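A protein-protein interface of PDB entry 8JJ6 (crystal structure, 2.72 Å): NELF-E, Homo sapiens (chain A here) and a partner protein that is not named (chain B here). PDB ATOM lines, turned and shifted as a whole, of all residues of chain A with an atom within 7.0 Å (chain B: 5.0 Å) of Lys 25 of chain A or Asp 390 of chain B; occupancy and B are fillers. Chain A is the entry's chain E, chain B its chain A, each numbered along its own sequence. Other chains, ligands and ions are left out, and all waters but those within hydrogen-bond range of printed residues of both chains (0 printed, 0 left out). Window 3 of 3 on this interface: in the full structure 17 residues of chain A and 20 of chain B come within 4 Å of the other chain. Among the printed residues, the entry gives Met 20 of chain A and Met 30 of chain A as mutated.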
ATOM      1  N   MET A  20     -24.766 -32.003  25.749  1.00  0.00           N
ATOM      2  CA  MET A  20     -25.516 -31.745  24.526  1.00  0.00           C
ATOM      3  C   MET A  20     -26.524 -30.632  24.740  1.00  0.00           C
ATOM      4  O   MET A  20     -26.723 -29.789  23.860  1.00  0.00           O
ATOM      5  CB  MET A  20     -26.197 -33.031  24.049  1.00  0.00           C
ATOM      6  CG  MET A  20     -25.194 -34.092  23.575  1.00  0.00           C
ATOM      7  SD  MET A  20     -25.872 -35.711  23.091  1.00  0.00           S
ATOM      8  CE  MET A  20     -26.283 -36.487  24.661  1.00  0.00           C
ATOM      9  N   LYS A  21     -27.144 -30.595  25.915  1.00  0.00           N
ATOM     10  CA  LYS A  21     -28.031 -29.489  26.232  1.00  0.00           C
ATOM     11  C   LYS A  21     -27.301 -28.161  26.104  1.00  0.00           C
ATOM     12  O   LYS A  21     -27.868 -27.183  25.614  1.00  0.00           O
ATOM     13  CB  LYS A  21     -28.610 -29.672  27.634  1.00  0.00           C
ATOM     14  CG  LYS A  21     -29.762 -28.738  27.950  1.00  0.00           C
ATOM     15  CD  LYS A  21     -30.294 -28.977  29.359  1.00  0.00           C
ATOM     16  CE  LYS A  21     -31.734 -28.511  29.489  1.00  0.00           C
ATOM     17  NZ  LYS A  21     -32.289 -28.769  30.853  1.00  0.00           N
ATOM     18  N   LEU A  22     -26.023 -28.124  26.493  1.00  0.00           N
ATOM     19  CA  LEU A  22     -25.235 -26.897  26.436  1.00  0.00           C
ATOM     20  C   LEU A  22     -24.770 -26.570  25.024  1.00  0.00           C
ATOM     21  O   LEU A  22     -24.572 -25.393  24.696  1.00  0.00           O
ATOM     22  CB  LEU A  22     -24.014 -27.008  27.349  1.00  0.00           C
ATOM     23  CG  LEU A  22     -23.171 -25.740  27.532  1.00  0.00           C
ATOM     24  CD1 LEU A  22     -24.054 -24.550  27.905  1.00  0.00           C
ATOM     25  CD2 LEU A  22     -22.086 -25.960  28.549  1.00  0.00           C
ATOM     26  N   LYS A  23     -24.556 -27.587  24.192  1.00  0.00           N
ATOM     27  CA  LYS A  23     -24.186 -27.325  22.808  1.00  0.00           C
ATOM     28  C   LYS A  23     -25.315 -26.595  22.093  1.00  0.00           C
ATOM     29  O   LYS A  23     -25.101 -25.534  21.494  1.00  0.00           O
ATOM     30  CB  LYS A  23     -23.843 -28.639  22.109  1.00  0.00           C
ATOM     31  CG  LYS A  23     -22.907 -28.500  20.936  1.00  0.00           C
ATOM     32  CD  LYS A  23     -22.260 -29.845  20.629  1.00  0.00           C
ATOM     33  CE  LYS A  23     -20.934 -29.685  19.866  1.00  0.00           C
ATOM     34  NZ  LYS A  23     -19.788 -29.177  20.699  1.00  0.00           N
ATOM     35  N   LYS A  24     -26.538 -27.136  22.197  1.00  0.00           N
ATOM     36  CA  LYS A  24     -27.713 -26.507  21.596  1.00  0.00           C
ATOM     37  C   LYS A  24     -27.862 -25.061  22.046  1.00  0.00           C
ATOM     38  O   LYS A  24     -28.037 -24.159  21.220  1.00  0.00           O
ATOM     39  CB  LYS A  24     -28.980 -27.291  21.953  1.00  0.00           C
ATOM     40  CG  LYS A  24     -29.085 -28.688  21.350  1.00  0.00           C
ATOM     41  CD  LYS A  24     -30.418 -29.318  21.737  1.00  0.00           C
ATOM     42  CE  LYS A  24     -30.347 -30.839  21.744  1.00  0.00           C
ATOM     43  NZ  LYS A  24     -31.509 -31.444  22.472  1.00  0.00           N
ATOM     44  N   LYS A  25     -27.811 -24.824  23.358  1.00  0.00           N
ATOM     45  CA  LYS A  25     -27.971 -23.468  23.866  1.00  0.00           C
ATOM     46  C   LYS A  25     -26.955 -22.528  23.242  1.00  0.00           C
ATOM     47  O   LYS A  25     -27.286 -21.389  22.892  1.00  0.00           O
ATOM     48  CB  LYS A  25     -27.830 -23.445  25.386  1.00  0.00           C
ATOM     49  CG  LYS A  25     -28.771 -24.348  26.118  1.00  0.00           C
ATOM     50  CD  LYS A  25     -29.847 -23.583  26.833  1.00  0.00           C
ATOM     51  CE  LYS A  25     -30.734 -24.531  27.602  1.00  0.00           C
ATOM     52  NZ  LYS A  25     -31.870 -23.791  28.178  1.00  0.00           N
ATOM     53  N   LYS A  26     -25.709 -22.991  23.091  1.00  0.00           N
ATOM     54  CA  LYS A  26     -24.651 -22.111  22.605  1.00  0.00           C
ATOM     55  C   LYS A  26     -24.785 -21.852  21.110  1.00  0.00           C
ATOM     56  O   LYS A  26     -24.378 -20.789  20.627  1.00  0.00           O
ATOM     57  CB  LYS A  26     -23.280 -22.706  22.940  1.00  0.00           C
ATOM     58  CG  LYS A  26     -22.552 -22.004  24.087  1.00  0.00           C
ATOM     59  CD  LYS A  26     -21.245 -22.704  24.451  1.00  0.00           C
ATOM     60  CE  LYS A  26     -20.414 -21.894  25.462  1.00  0.00           C
ATOM     61  NZ  LYS A  26     -19.755 -20.672  24.879  1.00  0.00           N
ATOM     62  N   LYS A  27     -25.363 -22.805  20.373  1.00  0.00           N
ATOM     63  CA  LYS A  27     -25.669 -22.570  18.966  1.00  0.00           C
ATOM     64  C   LYS A  27     -26.801 -21.563  18.824  1.00  0.00           C
ATOM     65  O   LYS A  27     -26.669 -20.565  18.111  1.00  0.00           O
ATOM     66  CB  LYS A  27     -26.018 -23.893  18.268  1.00  0.00           C
ATOM     67  CG  LYS A  27     -24.783 -24.728  17.929  1.00  0.00           C
ATOM     68  CD  LYS A  27     -25.014 -25.774  16.848  1.00  0.00           C
ATOM     69  CE  LYS A  27     -23.724 -25.959  16.028  1.00  0.00           C
ATOM     70  NZ  LYS A  27     -22.495 -26.034  16.892  1.00  0.00           N
ATOM     71  N   ALA A  28     -27.917 -21.801  19.523  1.00  0.00           N
ATOM     72  CA  ALA A  28     -29.021 -20.848  19.531  1.00  0.00           C
ATOM     73  C   ALA A  28     -28.573 -19.455  19.979  1.00  0.00           C
ATOM     74  O   ALA A  28     -29.113 -18.451  19.499  1.00  0.00           O
ATOM     75  CB  ALA A  28     -30.144 -21.367  20.429  1.00  0.00           C
ATOM     76  N   LEU A  29     -27.668 -19.355  20.922  1.00  0.00           N
ATOM     77  CA  LEU A  29     -27.178 -18.063  21.334  1.00  0.00           C
ATOM     78  C   LEU A  29     -26.433 -17.450  20.204  1.00  0.00           C
ATOM     79  O   LEU A  29     -26.439 -16.268  20.013  1.00  0.00           O
ATOM     80  CB  LEU A  29     -26.221 -18.194  22.496  1.00  0.00           C
ATOM     81  CG  LEU A  29     -25.899 -16.903  23.223  1.00  0.00           C
ATOM     82  CD1 LEU A  29     -24.481 -16.415  22.991  1.00  0.00           C
ATOM     83  CD2 LEU A  29     -26.911 -15.868  22.828  1.00  0.00           C
ATOM     84  N   MET A  30     -25.724 -18.274  19.474  1.00  0.00           N
ATOM     85  CA  MET A  30     -24.933 -17.771  18.386  1.00  0.00           C
ATOM     86  C   MET A  30     -25.757 -17.097  17.302  1.00  0.00           C
ATOM     87  O   MET A  30     -25.392 -16.048  16.810  1.00  0.00           O
ATOM     88  CB  MET A  30     -24.114 -18.908  17.793  1.00  0.00           C
ATOM     89  CG  MET A  30     -22.979 -18.469  16.905  1.00  0.00           C
ATOM     90  SD  MET A  30     -23.287 -18.947  15.195  1.00  0.00           S
ATOM     91  CE  MET A  30     -21.874 -18.319  14.300  1.00  0.00           C
ATOM     92  N   THR B 386     -24.583 -23.630  31.585  1.00  0.00           N
ATOM     93  CA  THR B 386     -25.907 -23.561  30.980  1.00  0.00           C
ATOM     94  C   THR B 386     -26.730 -22.428  31.591  1.00  0.00           C
ATOM     95  O   THR B 386     -27.463 -21.733  30.878  1.00  0.00           O
ATOM     96  CB  THR B 386     -26.625 -24.910  31.111  1.00  0.00           C
ATOM     97  OG1 THR B 386     -25.816 -25.954  30.544  1.00  0.00           O
ATOM     98  CG2 THR B 386     -27.961 -24.876  30.387  1.00  0.00           C
ATOM     99  N   PHE B 387     -26.599 -22.195  32.898  1.00  0.00           N
ATOM    100  CA  PHE B 387     -27.297 -21.068  33.510  1.00  0.00           C
ATOM    101  C   PHE B 387     -26.857 -19.746  32.892  1.00  0.00           C
ATOM    102  O   PHE B 387     -27.695 -18.902  32.554  1.00  0.00           O
ATOM    103  CB  PHE B 387     -27.069 -21.051  35.020  1.00  0.00           C
ATOM    104  CG  PHE B 387     -27.789 -19.936  35.732  1.00  0.00           C
ATOM    105  CD1 PHE B 387     -29.129 -20.065  36.066  1.00  0.00           C
ATOM    106  CD2 PHE B 387     -27.124 -18.762  36.071  1.00  0.00           C
ATOM    107  CE1 PHE B 387     -29.795 -19.045  36.728  1.00  0.00           C
ATOM    108  CE2 PHE B 387     -27.777 -17.738  36.728  1.00  0.00           C
ATOM    109  CZ  PHE B 387     -29.116 -17.878  37.060  1.00  0.00           C
ATOM    110  N   ASN B 388     -25.542 -19.546  32.742  1.00  0.00           N
ATOM    111  CA  ASN B 388     -25.032 -18.315  32.140  1.00  0.00           C
ATOM    112  C   ASN B 388     -25.641 -18.072  30.758  1.00  0.00           C
ATOM    113  O   ASN B 388     -26.085 -16.960  30.446  1.00  0.00           O
ATOM    114  CB  ASN B 388     -23.510 -18.377  32.045  1.00  0.00           C
ATOM    115  CG  ASN B 388     -22.833 -18.257  33.397  1.00  0.00           C
ATOM    116  OD1 ASN B 388     -23.498 -18.249  34.438  1.00  0.00           O
ATOM    117  ND2 ASN B 388     -21.494 -18.163  33.390  1.00  0.00           N
ATOM    118  N   VAL B 389     -25.669 -19.104  29.911  1.00  0.00           N
ATOM    119  CA  VAL B 389     -26.207 -18.939  28.566  1.00  0.00           C
ATOM    120  C   VAL B 389     -27.731 -18.805  28.601  1.00  0.00           C
ATOM    121  O   VAL B 389     -28.320 -18.096  27.778  1.00  0.00           O
ATOM    122  CB  VAL B 389     -25.736 -20.110  27.679  1.00  0.00           C
ATOM    123  CG1 VAL B 389     -26.714 -20.369  26.555  1.00  0.00           C
ATOM    124  CG2 VAL B 389     -24.346 -19.828  27.119  1.00  0.00           C
ATOM    125  N   ASP B 390     -28.392 -19.452  29.561  1.00  0.00           N
ATOM    126  CA  ASP B 390     -29.835 -19.279  29.705  1.00  0.00           C
ATOM    127  C   ASP B 390     -30.204 -17.830  29.999  1.00  0.00           C
ATOM    128  O   ASP B 390     -31.307 -17.388  29.659  1.00  0.00           O
ATOM    129  CB  ASP B 390     -30.365 -20.185  30.815  1.00  0.00           C
ATOM    130  CG  ASP B 390     -30.910 -21.496  30.285  1.00  0.00           C
ATOM    131  OD1 ASP B 390     -30.906 -21.672  29.042  1.00  0.00           O
ATOM    132  OD2 ASP B 390     -31.330 -22.349  31.108  1.00  0.00           O
ATOM    133  N   GLN B 391     -29.308 -17.072  30.624  1.00  0.00           N
ATOM    134  CA  GLN B 391     -29.638 -15.680  30.891  1.00  0.00           C
ATOM    135  C   GLN B 391     -29.436 -14.815  29.653  1.00  0.00           C
ATOM    136  O   GLN B 391     -30.231 -13.906  29.393  1.00  0.00           O
ATOM    137  CB  GLN B 391     -28.818 -15.163  32.069  1.00  0.00           C
ATOM    138  CG  GLN B 391     -29.065 -15.968  33.319  1.00  0.00           C
ATOM    139  CD  GLN B 391     -29.668 -15.144  34.436  1.00  0.00           C
ATOM    140  OE1 GLN B 391     -28.951 -14.508  35.219  1.00  0.00           O
ATOM    141  NE2 GLN B 391     -31.000 -15.141  34.515  1.00  0.00           N
ATOM    142  N   LYS B 392     -28.394 -15.091  28.865  1.00  0.00           N
ATOM    143  CA  LYS B 392     -28.141 -14.329  27.643  1.00  0.00           C
ATOM    144  C   LYS B 392     -29.158 -14.652  26.543  1.00  0.00           C
ATOM    145  O   LYS B 392     -28.989 -14.253  25.383  1.00  0.00           O
ATOM    146  CB  LYS B 392     -26.711 -14.584  27.140  1.00  0.00           C
ATOM    147  CG  LYS B 392     -25.640 -13.679  27.731  1.00  0.00           C
ATOM    148  CD  LYS B 392     -24.261 -14.370  27.759  1.00  0.00           C
ATOM    149  CE  LYS B 392     -23.132 -13.401  28.062  1.00  0.00           C
ATOM    150  NZ  LYS B 392     -22.909 -12.403  26.968  1.00  0.00           N
ATOM    151  N   LEU B 393     -30.207 -15.391  26.887  1.00  0.00           N
ATOM    152  CA  LEU B 393     -31.214 -15.686  25.894  1.00  0.00           C
ATOM    153  C   LEU B 393     -32.517 -14.975  26.228  1.00  0.00           C
ATOM    154  O   LEU B 393     -32.871 -14.829  27.403  1.00  0.00           O
ATOM    155  CB  LEU B 393     -31.466 -17.192  25.775  1.00  0.00           C
ATOM    156  CG  LEU B 393     -30.390 -17.940  24.975  1.00  0.00           C
ATOM    157  CD1 LEU B 393     -30.693 -19.424  24.948  1.00  0.00           C
ATOM    158  CD2 LEU B 393     -30.251 -17.382  23.564  1.00  0.00           C
ATOM    159  N   GLU B 396     -37.397 -15.190  28.562  1.00  0.00           N
ATOM    160  CA  GLU B 396     -37.417 -16.025  29.757  1.00  0.00           C
ATOM    161  C   GLU B 396     -38.843 -16.429  30.116  1.00  0.00           C
ATOM    162  O   GLU B 396     -39.052 -17.491  30.719  1.00  0.00           O
ATOM    163  CB  GLU B 396     -36.751 -15.289  30.930  1.00  0.00           C
ATOM    164  CG  GLU B 396     -35.251 -15.569  31.102  1.00  0.00           C
ATOM    165  CD  GLU B 396     -34.506 -14.449  31.832  1.00  0.00           C
ATOM    166  OE1 GLU B 396     -34.404 -14.508  33.080  1.00  0.00           O
ATOM    167  OE2 GLU B 396     -34.014 -13.517  31.152  1.00  0.00           O
ATOM    168  N   VAL B 401     -35.163 -18.904  34.497  1.00  0.00           N
ATOM    169  CA  VAL B 401     -34.542 -20.091  35.083  1.00  0.00           C
ATOM    170  C   VAL B 401     -34.021 -19.861  36.502  1.00  0.00           C
ATOM    171  O   VAL B 401     -33.325 -18.877  36.777  1.00  0.00           O
ATOM    172  CB  VAL B 401     -33.418 -20.606  34.161  1.00  0.00           C
ATOM    173  CG1 VAL B 401     -32.465 -19.465  33.773  1.00  0.00           C
ATOM    174  CG2 VAL B 401     -32.677 -21.791  34.810  1.00  0.00           C
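Of the 10 printed residues of chain B, 5 touch a printed residue of chain A.
Printed residues of chain B that touch a printed residue of chain A: Thr 386, Val 389, Asp 390, Lys 392 and Leu 393.
Hydrophobic or aromatic side chains of chain A that line the printed part of chain B: Leu 22 and Leu 29.
Among the printed residues, 6 pairs touch across the chains.
Among the printed residues, Asp or Glu carboxylates within 4 Å of a Lys or Arg side-chain nitrogen of the other chain: Lys 25 of chain A with Asp 390 of chain B.
The side-chain amino group (NZ) of Lys 25 of chain A is in salt-bridge range of the side-chain carboxylate (OD1) of Asp 390 of chain B, 2.5 Å away.
Printed residues of chain B within 4 Å of Leu 29 of chain A: Lys 392 and Leu 393.
Printed residues of chain A within 4 Å of Val 389 of chain B: Lys 25 (3.5 Å).
Printed residues of chain A within 4 Å of Asp 390 of chain B: Lys 25 (2.5 Å).
The nearest residue of chain A that does not touch Asp 390 of chain B is Lys 21 of chain A (6.4 Å).
The nearest printed residue of chain A that does not touch Lys 392 of chain B is Ala 28 of chain A (7.2 Å).
Leu 22 of chain A touches Thr 386 of chain B (CD1 to OG1, 3.5 Å).
Thr 386 of chain B touches Lys 25 of chain A (CG2 to CE, 3.9 Å).
Lys 25 of chain A touches Val 389 of chain B (CB to CG1, 3.5 Å).
Lys 392 of chain B touches Leu 29 of chain A (O to CD2, 3.7 Å).
CD2 of Leu 29 of chain A touches CD2 of Leu 393 of chain B (3.7 Å).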
